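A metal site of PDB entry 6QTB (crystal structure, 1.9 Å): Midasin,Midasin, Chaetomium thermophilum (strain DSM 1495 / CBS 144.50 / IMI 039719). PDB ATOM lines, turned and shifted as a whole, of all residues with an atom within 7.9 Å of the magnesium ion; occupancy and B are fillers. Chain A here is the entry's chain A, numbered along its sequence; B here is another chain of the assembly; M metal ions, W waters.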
ATOM      1  N   ASP A  62       6.477 -17.195 -22.538  1.00  0.00           N
ATOM      2  CA  ASP A  62       5.255 -16.448 -22.243  1.00  0.00           C
ATOM      3  C   ASP A  62       5.215 -16.055 -20.767  1.00  0.00           C
ATOM      4  O   ASP A  62       5.225 -16.911 -19.886  1.00  0.00           O
ATOM      5  CB  ASP A  62       4.083 -17.370 -22.599  1.00  0.00           C
ATOM      6  CG  ASP A  62       2.712 -16.678 -22.570  1.00  0.00           C
ATOM      7  OD1 ASP A  62       2.520 -15.772 -21.752  1.00  0.00           O
ATOM      8  OD2 ASP A  62       1.862 -17.089 -23.431  1.00  0.00           O
ATOM      9  N   ASP A  63       5.232 -14.721 -20.513  1.00  0.00           N
ATOM     10  CA  ASP A  63       5.198 -14.175 -19.174  1.00  0.00           C
ATOM     11  C   ASP A  63       3.798 -13.637 -18.828  1.00  0.00           C
ATOM     12  O   ASP A  63       3.666 -12.831 -17.869  1.00  0.00           O
ATOM     13  CB  ASP A  63       6.267 -13.028 -19.059  1.00  0.00           C
ATOM     14  CG  ASP A  63       6.498 -12.560 -17.647  1.00  0.00           C
ATOM     15  OD1 ASP A  63       6.649 -13.403 -16.731  1.00  0.00           O
ATOM     16  OD2 ASP A  63       6.554 -11.287 -17.437  1.00  0.00           O
ATOM     17  N   SER A  64       2.770 -14.003 -19.606  1.00  0.00           N
ATOM     18  CA  SER A  64       1.415 -13.525 -19.355  1.00  0.00           C
ATOM     19  C   SER A  64       0.742 -14.237 -18.164  1.00  0.00           C
ATOM     20  O   SER A  64       1.084 -15.351 -17.777  1.00  0.00           O
ATOM     21  CB  SER A  64       0.525 -13.675 -20.625  1.00  0.00           C
ATOM     22  OG  SER A  64       0.180 -15.046 -20.895  1.00  0.00           O
ATOM     23  N   SER A  65      -0.274 -13.572 -17.579  1.00  0.00           N
ATOM     24  CA  SER A  65      -0.814 -14.158 -16.363  1.00  0.00           C
ATOM     25  C   SER A  65      -1.769 -15.350 -16.655  1.00  0.00           C
ATOM     26  O   SER A  65      -2.087 -16.088 -15.722  1.00  0.00           O
ATOM     27  CB  SER A  65      -1.501 -13.048 -15.528  1.00  0.00           C
ATOM     28  OG  SER A  65      -2.682 -12.703 -16.129  1.00  0.00           O
ATOM     29  N   SER A  66      -2.080 -15.657 -17.902  1.00  0.00           N
ATOM     30  CA  SER A  66      -2.807 -16.926 -18.159  1.00  0.00           C
ATOM     31  C   SER A  66      -1.940 -18.143 -17.808  1.00  0.00           C
ATOM     32  O   SER A  66      -2.447 -19.242 -17.534  1.00  0.00           O
ATOM     33  CB  SER A  66      -3.234 -17.041 -19.624  1.00  0.00           C
ATOM     34  OG  SER A  66      -2.080 -16.978 -20.484  1.00  0.00           O
ATOM     35  N   MET A  67      -0.638 -17.943 -17.745  1.00  0.00           N
ATOM     36  CA  MET A  67       0.314 -18.992 -17.446  1.00  0.00           C
ATOM     37  C   MET A  67       0.335 -19.333 -15.965  1.00  0.00           C
ATOM     38  O   MET A  67       0.892 -20.362 -15.570  1.00  0.00           O
ATOM     39  CB  MET A  67       1.738 -18.530 -17.885  1.00  0.00           C
ATOM     40  CG  MET A  67       1.871 -18.109 -19.380  1.00  0.00           C
ATOM     41  SD  MET A  67       1.906 -19.640 -20.448  1.00  0.00           S
ATOM     42  CE  MET A  67       3.578 -20.321 -20.204  1.00  0.00           C
ATOM     43  N   SER A  68      -0.262 -18.471 -15.125  1.00  0.00           N
ATOM     44  CA  SER A  68       0.123 -18.395 -13.723  1.00  0.00           C
ATOM     45  C   SER A  68      -0.705 -19.286 -12.812  1.00  0.00           C
ATOM     46  O   SER A  68      -1.879 -19.536 -13.049  1.00  0.00           O
ATOM     47  CB  SER A  68      -0.049 -16.951 -13.224  1.00  0.00           C
ATOM     48  OG  SER A  68       0.073 -16.952 -11.819  1.00  0.00           O
ATOM     49  N   ASN A  71      -4.007 -18.131 -11.785  1.00  0.00           N
ATOM     50  CA  ASN A  71      -5.053 -18.474 -12.725  1.00  0.00           C
ATOM     51  C   ASN A  71      -5.357 -19.974 -12.719  1.00  0.00           C
ATOM     52  O   ASN A  71      -6.024 -20.456 -13.636  1.00  0.00           O
ATOM     53  CB  ASN A  71      -4.659 -18.035 -14.142  1.00  0.00           C
ATOM     54  CG  ASN A  71      -5.828 -18.108 -15.138  1.00  0.00           C
ATOM     55  OD1 ASN A  71      -6.919 -17.625 -14.868  1.00  0.00           O
ATOM     56  ND2 ASN A  71      -5.594 -18.741 -16.291  1.00  0.00           N
ATOM     57  N   PHE A 103       7.728 -12.550 -22.854  1.00  0.00           N
ATOM     58  CA  PHE A 103       6.776 -11.677 -23.558  1.00  0.00           C
ATOM     59  C   PHE A 103       5.387 -11.718 -22.921  1.00  0.00           C
ATOM     60  O   PHE A 103       4.964 -12.730 -22.387  1.00  0.00           O
ATOM     61  CB  PHE A 103       6.673 -12.055 -25.043  1.00  0.00           C
ATOM     62  CG  PHE A 103       6.050 -13.424 -25.325  1.00  0.00           C
ATOM     63  CD1 PHE A 103       6.858 -14.605 -25.352  1.00  0.00           C
ATOM     64  CD2 PHE A 103       4.691 -13.545 -25.577  1.00  0.00           C
ATOM     65  CE1 PHE A 103       6.305 -15.868 -25.648  1.00  0.00           C
ATOM     66  CE2 PHE A 103       4.135 -14.819 -25.820  1.00  0.00           C
ATOM     67  CZ  PHE A 103       4.927 -15.954 -25.858  1.00  0.00           C
ATOM     68  N   GLY A 104       4.705 -10.588 -22.975  1.00  0.00           N
ATOM     69  CA  GLY A 104       3.266 -10.567 -22.616  1.00  0.00           C
ATOM     70  C   GLY A 104       2.680  -9.351 -23.293  1.00  0.00           C
ATOM     71  O   GLY A 104       2.401  -9.380 -24.497  1.00  0.00           O
ATOM     72  N   GLN A 135       1.766 -10.542 -16.610  1.00  0.00           N
ATOM     73  CA  GLN A 135       1.376  -9.540 -17.618  1.00  0.00           C
ATOM     74  C   GLN A 135      -0.073  -9.675 -18.040  1.00  0.00           C
ATOM     75  O   GLN A 135      -0.635 -10.767 -18.086  1.00  0.00           O
ATOM     76  CB  GLN A 135       2.295  -9.582 -18.837  1.00  0.00           C
ATOM     77  CG  GLN A 135       3.767  -9.258 -18.379  1.00  0.00           C
ATOM     78  CD  GLN A 135       4.667  -8.812 -19.504  1.00  0.00           C
ATOM     79  OE1 GLN A 135       4.262  -8.035 -20.345  1.00  0.00           O
ATOM     80  NE2 GLN A 135       5.917  -9.374 -19.545  1.00  0.00           N
ATOM     81  N   ASP A 136      -0.690  -8.532 -18.371  1.00  0.00           N
ATOM     82  CA  ASP A 136      -2.125  -8.481 -18.604  1.00  0.00           C
ATOM     83  C   ASP A 136      -2.557  -8.803 -20.027  1.00  0.00           C
ATOM     84  O   ASP A 136      -3.739  -8.658 -20.318  1.00  0.00           O
ATOM     85  CB  ASP A 136      -2.672  -7.082 -18.231  1.00  0.00           C
ATOM     86  CG  ASP A 136      -2.631  -6.831 -16.738  1.00  0.00           C
ATOM     87  OD1 ASP A 136      -2.656  -7.817 -15.957  1.00  0.00           O
ATOM     88  OD2 ASP A 136      -2.553  -5.652 -16.355  1.00  0.00           O
ATOM     89  N   SER A 137      -1.654  -9.156 -20.930  1.00  0.00           N
ATOM     90  CA  SER A 137      -2.073  -9.519 -22.262  1.00  0.00           C
ATOM     91  C   SER A 137      -1.008 -10.429 -22.861  1.00  0.00           C
ATOM     92  O   SER A 137       0.085 -10.606 -22.293  1.00  0.00           O
ATOM     93  CB  SER A 137      -2.352  -8.296 -23.171  1.00  0.00           C
ATOM     94  OG  SER A 137      -1.146  -7.614 -23.460  1.00  0.00           O
ATOM     95  N   THR A 138      -1.351 -11.045 -23.993  1.00  0.00           N
ATOM     96  CA  THR A 138      -0.414 -12.012 -24.607  1.00  0.00           C
ATOM     97  C   THR A 138      -0.229 -11.573 -26.053  1.00  0.00           C
ATOM     98  O   THR A 138      -0.930 -12.029 -26.950  1.00  0.00           O
ATOM     99  CB  THR A 138      -0.943 -13.433 -24.491  1.00  0.00           C
ATOM    100  OG1 THR A 138      -1.217 -13.753 -23.102  1.00  0.00           O
ATOM    101  CG2 THR A 138       0.120 -14.453 -25.093  1.00  0.00           C
ATOM    102  N   ASP A 139       0.712 -10.672 -26.315  1.00  0.00           N
ATOM    103  CA  ASP A 139       0.784 -10.046 -27.669  1.00  0.00           C
ATOM    104  C   ASP A 139       1.752 -10.810 -28.578  1.00  0.00           C
ATOM    105  O   ASP A 139       2.938 -10.505 -28.739  1.00  0.00           O
ATOM    106  CB  ASP A 139       1.180  -8.589 -27.527  1.00  0.00           C
ATOM    107  CG  ASP A 139       1.012  -7.794 -28.830  1.00  0.00           C
ATOM    108  OD1 ASP A 139       0.871  -8.434 -29.889  1.00  0.00           O
ATOM    109  OD2 ASP A 139       1.092  -6.534 -28.759  1.00  0.00           O
ATOM    110  N   MET A 140       1.225 -11.879 -29.199  1.00  0.00           N
ATOM    111  CA  MET A 140       2.073 -12.766 -29.997  1.00  0.00           C
ATOM    112  C   MET A 140       2.556 -12.093 -31.269  1.00  0.00           C
ATOM    113  O   MET A 140       3.590 -12.494 -31.811  1.00  0.00           O
ATOM    114  CB  MET A 140       1.268 -14.065 -30.315  1.00  0.00           C
ATOM    115  CG  MET A 140       2.127 -15.266 -30.752  1.00  0.00           C
ATOM    116  SD  MET A 140       3.105 -15.920 -29.398  1.00  0.00           S
ATOM    117  CE  MET A 140       1.872 -16.640 -28.324  1.00  0.00           C
ATOM    118  N   SER A 176       4.763 -21.585 -24.341  1.00  0.00           N
ATOM    119  CA  SER A 176       3.551 -20.790 -24.092  1.00  0.00           C
ATOM    120  C   SER A 176       2.390 -21.742 -23.967  1.00  0.00           C
ATOM    121  O   SER A 176       2.428 -22.848 -24.536  1.00  0.00           O
ATOM    122  CB  SER A 176       3.323 -19.791 -25.254  1.00  0.00           C
ATOM    123  OG  SER A 176       2.051 -19.107 -25.216  1.00  0.00           O
ATOM    124  N   ASP A 177       1.321 -21.280 -23.247  1.00  0.00           N
ATOM    125  CA  ASP A 177       0.081 -22.059 -23.247  1.00  0.00           C
ATOM    126  C   ASP A 177      -0.676 -21.938 -24.566  1.00  0.00           C
ATOM    127  O   ASP A 177      -1.677 -22.651 -24.768  1.00  0.00           O
ATOM    128  CB  ASP A 177      -0.822 -21.638 -22.044  1.00  0.00           C
ATOM    129  CG  ASP A 177      -1.224 -20.101 -22.089  1.00  0.00           C
ATOM    130  OD1 ASP A 177      -1.107 -19.463 -23.168  1.00  0.00           O
ATOM    131  OD2 ASP A 177      -1.617 -19.569 -21.002  1.00  0.00           O
ATOM    132  N   GLY A 178      -0.217 -21.087 -25.490  1.00  0.00           N
ATOM    133  CA  GLY A 178      -0.834 -21.003 -26.797  1.00  0.00           C
ATOM    134  C   GLY A 178      -2.184 -20.297 -26.880  1.00  0.00           C
ATOM    135  O   GLY A 178      -2.806 -20.345 -27.950  1.00  0.00           O
ATOM    136  N   LEU A 179      -2.585 -19.549 -25.830  1.00  0.00           N
ATOM    137  CA  LEU A 179      -3.898 -18.889 -25.744  1.00  0.00           C
ATOM    138  C   LEU A 179      -3.728 -17.448 -26.199  1.00  0.00           C
ATOM    139  O   LEU A 179      -3.177 -16.598 -25.487  1.00  0.00           O
ATOM    140  CB  LEU A 179      -4.377 -18.955 -24.310  1.00  0.00           C
ATOM    141  CG  LEU A 179      -4.663 -20.338 -23.711  1.00  0.00           C
ATOM    142  CD1 LEU A 179      -4.981 -20.256 -22.198  1.00  0.00           C
ATOM    143  CD2 LEU A 179      -5.834 -21.040 -24.432  1.00  0.00           C
ATOM    144  N   VAL A 180      -4.123 -17.182 -27.410  1.00  0.00           N
ATOM    145  CA  VAL A 180      -4.102 -15.837 -27.930  1.00  0.00           C
ATOM    146  C   VAL A 180      -5.508 -15.563 -28.419  1.00  0.00           C
ATOM    147  O   VAL A 180      -6.283 -16.487 -28.698  1.00  0.00           O
ATOM    148  CB  VAL A 180      -3.054 -15.603 -29.023  1.00  0.00           C
ATOM    149  CG1 VAL A 180      -1.619 -16.030 -28.494  1.00  0.00           C
ATOM    150  CG2 VAL A 180      -3.352 -16.352 -30.291  1.00  0.00           C
ATOM    151  N   SER B  89      -7.846  -9.208 -15.793  1.00  0.00           N
ATOM    152  CA  SER B  89      -7.670  -8.985 -17.227  1.00  0.00           C
ATOM    153  C   SER B  89      -8.328 -10.102 -18.010  1.00  0.00           C
ATOM    154  O   SER B  89      -8.815 -11.089 -17.462  1.00  0.00           O
ATOM    155  CB  SER B  89      -6.193  -8.893 -17.618  1.00  0.00           C
ATOM    156  OG  SER B  89      -5.644 -10.222 -17.630  1.00  0.00           O
ATOM    157  N   LEU B  90      -8.285  -9.934 -19.348  1.00  0.00           N
ATOM    158  CA  LEU B  90      -8.780 -10.988 -20.244  1.00  0.00           C
ATOM    159  C   LEU B  90      -7.950 -12.268 -20.168  1.00  0.00           C
ATOM    160  O   LEU B  90      -8.346 -13.295 -20.750  1.00  0.00           O
ATOM    161  CB  LEU B  90      -8.797 -10.442 -21.674  1.00  0.00           C
ATOM    162  CG  LEU B  90      -9.824  -9.299 -21.827  1.00  0.00           C
ATOM    163  CD1 LEU B  90      -9.760  -8.621 -23.181  1.00  0.00           C
ATOM    164  CD2 LEU B  90     -11.282  -9.822 -21.611  1.00  0.00           C
ATOM    165  N   GLU B  91      -6.783 -12.252 -19.473  1.00  0.00           N
ATOM    166  CA  GLU B  91      -5.978 -13.481 -19.277  1.00  0.00           C
ATOM    167  C   GLU B  91      -6.634 -14.459 -18.288  1.00  0.00           C
ATOM    168  O   GLU B  91      -6.187 -15.612 -18.183  1.00  0.00           O
ATOM    169  CB  GLU B  91      -4.593 -13.131 -18.716  1.00  0.00           C
ATOM    170  CG  GLU B  91      -3.772 -12.228 -19.610  1.00  0.00           C
ATOM    171  CD  GLU B  91      -3.115 -13.046 -20.775  1.00  0.00           C
ATOM    172  OE1 GLU B  91      -2.545 -14.160 -20.488  1.00  0.00           O
ATOM    173  OE2 GLU B  91      -3.204 -12.531 -21.905  1.00  0.00           O
ATOM    174  N   THR B  92      -7.666 -14.014 -17.557  1.00  0.00           N
ATOM    175  CA  THR B  92      -8.238 -14.814 -16.478  1.00  0.00           C
ATOM    176  C   THR B  92      -9.229 -15.839 -17.030  1.00  0.00           C
ATOM    177  O   THR B  92     -10.137 -15.481 -17.787  1.00  0.00           O
ATOM    178  CB  THR B  92      -8.997 -13.911 -15.500  1.00  0.00           C
ATOM    179  OG1 THR B  92      -8.128 -12.859 -15.078  1.00  0.00           O
ATOM    180  CG2 THR B  92      -9.545 -14.690 -14.264  1.00  0.00           C
HETATM  181 MG    MG M   1      -1.559 -15.415 -21.881  1.00  0.00          MG
HETATM  182  O   HOH W   1      -0.647 -16.850 -22.961  1.00  0.00           O
HETATM  183  O   HOH W   2      -3.383 -15.811 -22.962  1.00  0.00           O
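Water W1 binds the magnesium ion (2.0 Å).
OG of Ser 64 binds the magnesium ion, 2.0 Å away.
The magnesium ion is bound by OG1 of Thr 138 (2.1 Å).
OE1 of Glu 91 of chain B is bound to the magnesium ion.
The magnesium ion is bound by water W2, at 2.2 Å.
OG of Ser 66 is bound to the magnesium ion, at 2.2 Å.
Water W2 bridges the backbone carbonyl oxygen (O) of Leu 179 and the side-chain carboxylate (OE2) of Glu 91 of chain B.
Water W1 lies within hydrogen-bond range of the side-chain carboxylate (OD2) of Asp 62 (2.6 Å) and the side-chain carboxylate (OD1) of Asp 177 (2.7 Å).
Of the 25 residues printed, 4 come within 4 Å of the magnesium ion.
The backbone NH (N) of Ser 64 lies within hydrogen-bond range of the side-chain carboxylate (OD1) of Asp 62.
OG of Ser 89 of chain B is in hydrogen-bond range of N of Glu 91 of chain B, 3.0 Å away.
The side-chain hydroxyl (OG) of Ser 66 sits close to the side-chain carboxylate (OD2) of Asp 177, at 2.7 Å.
O of Ser 66 is in hydrogen-bond range of ND2 of Asn 71, 3.4 Å away.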
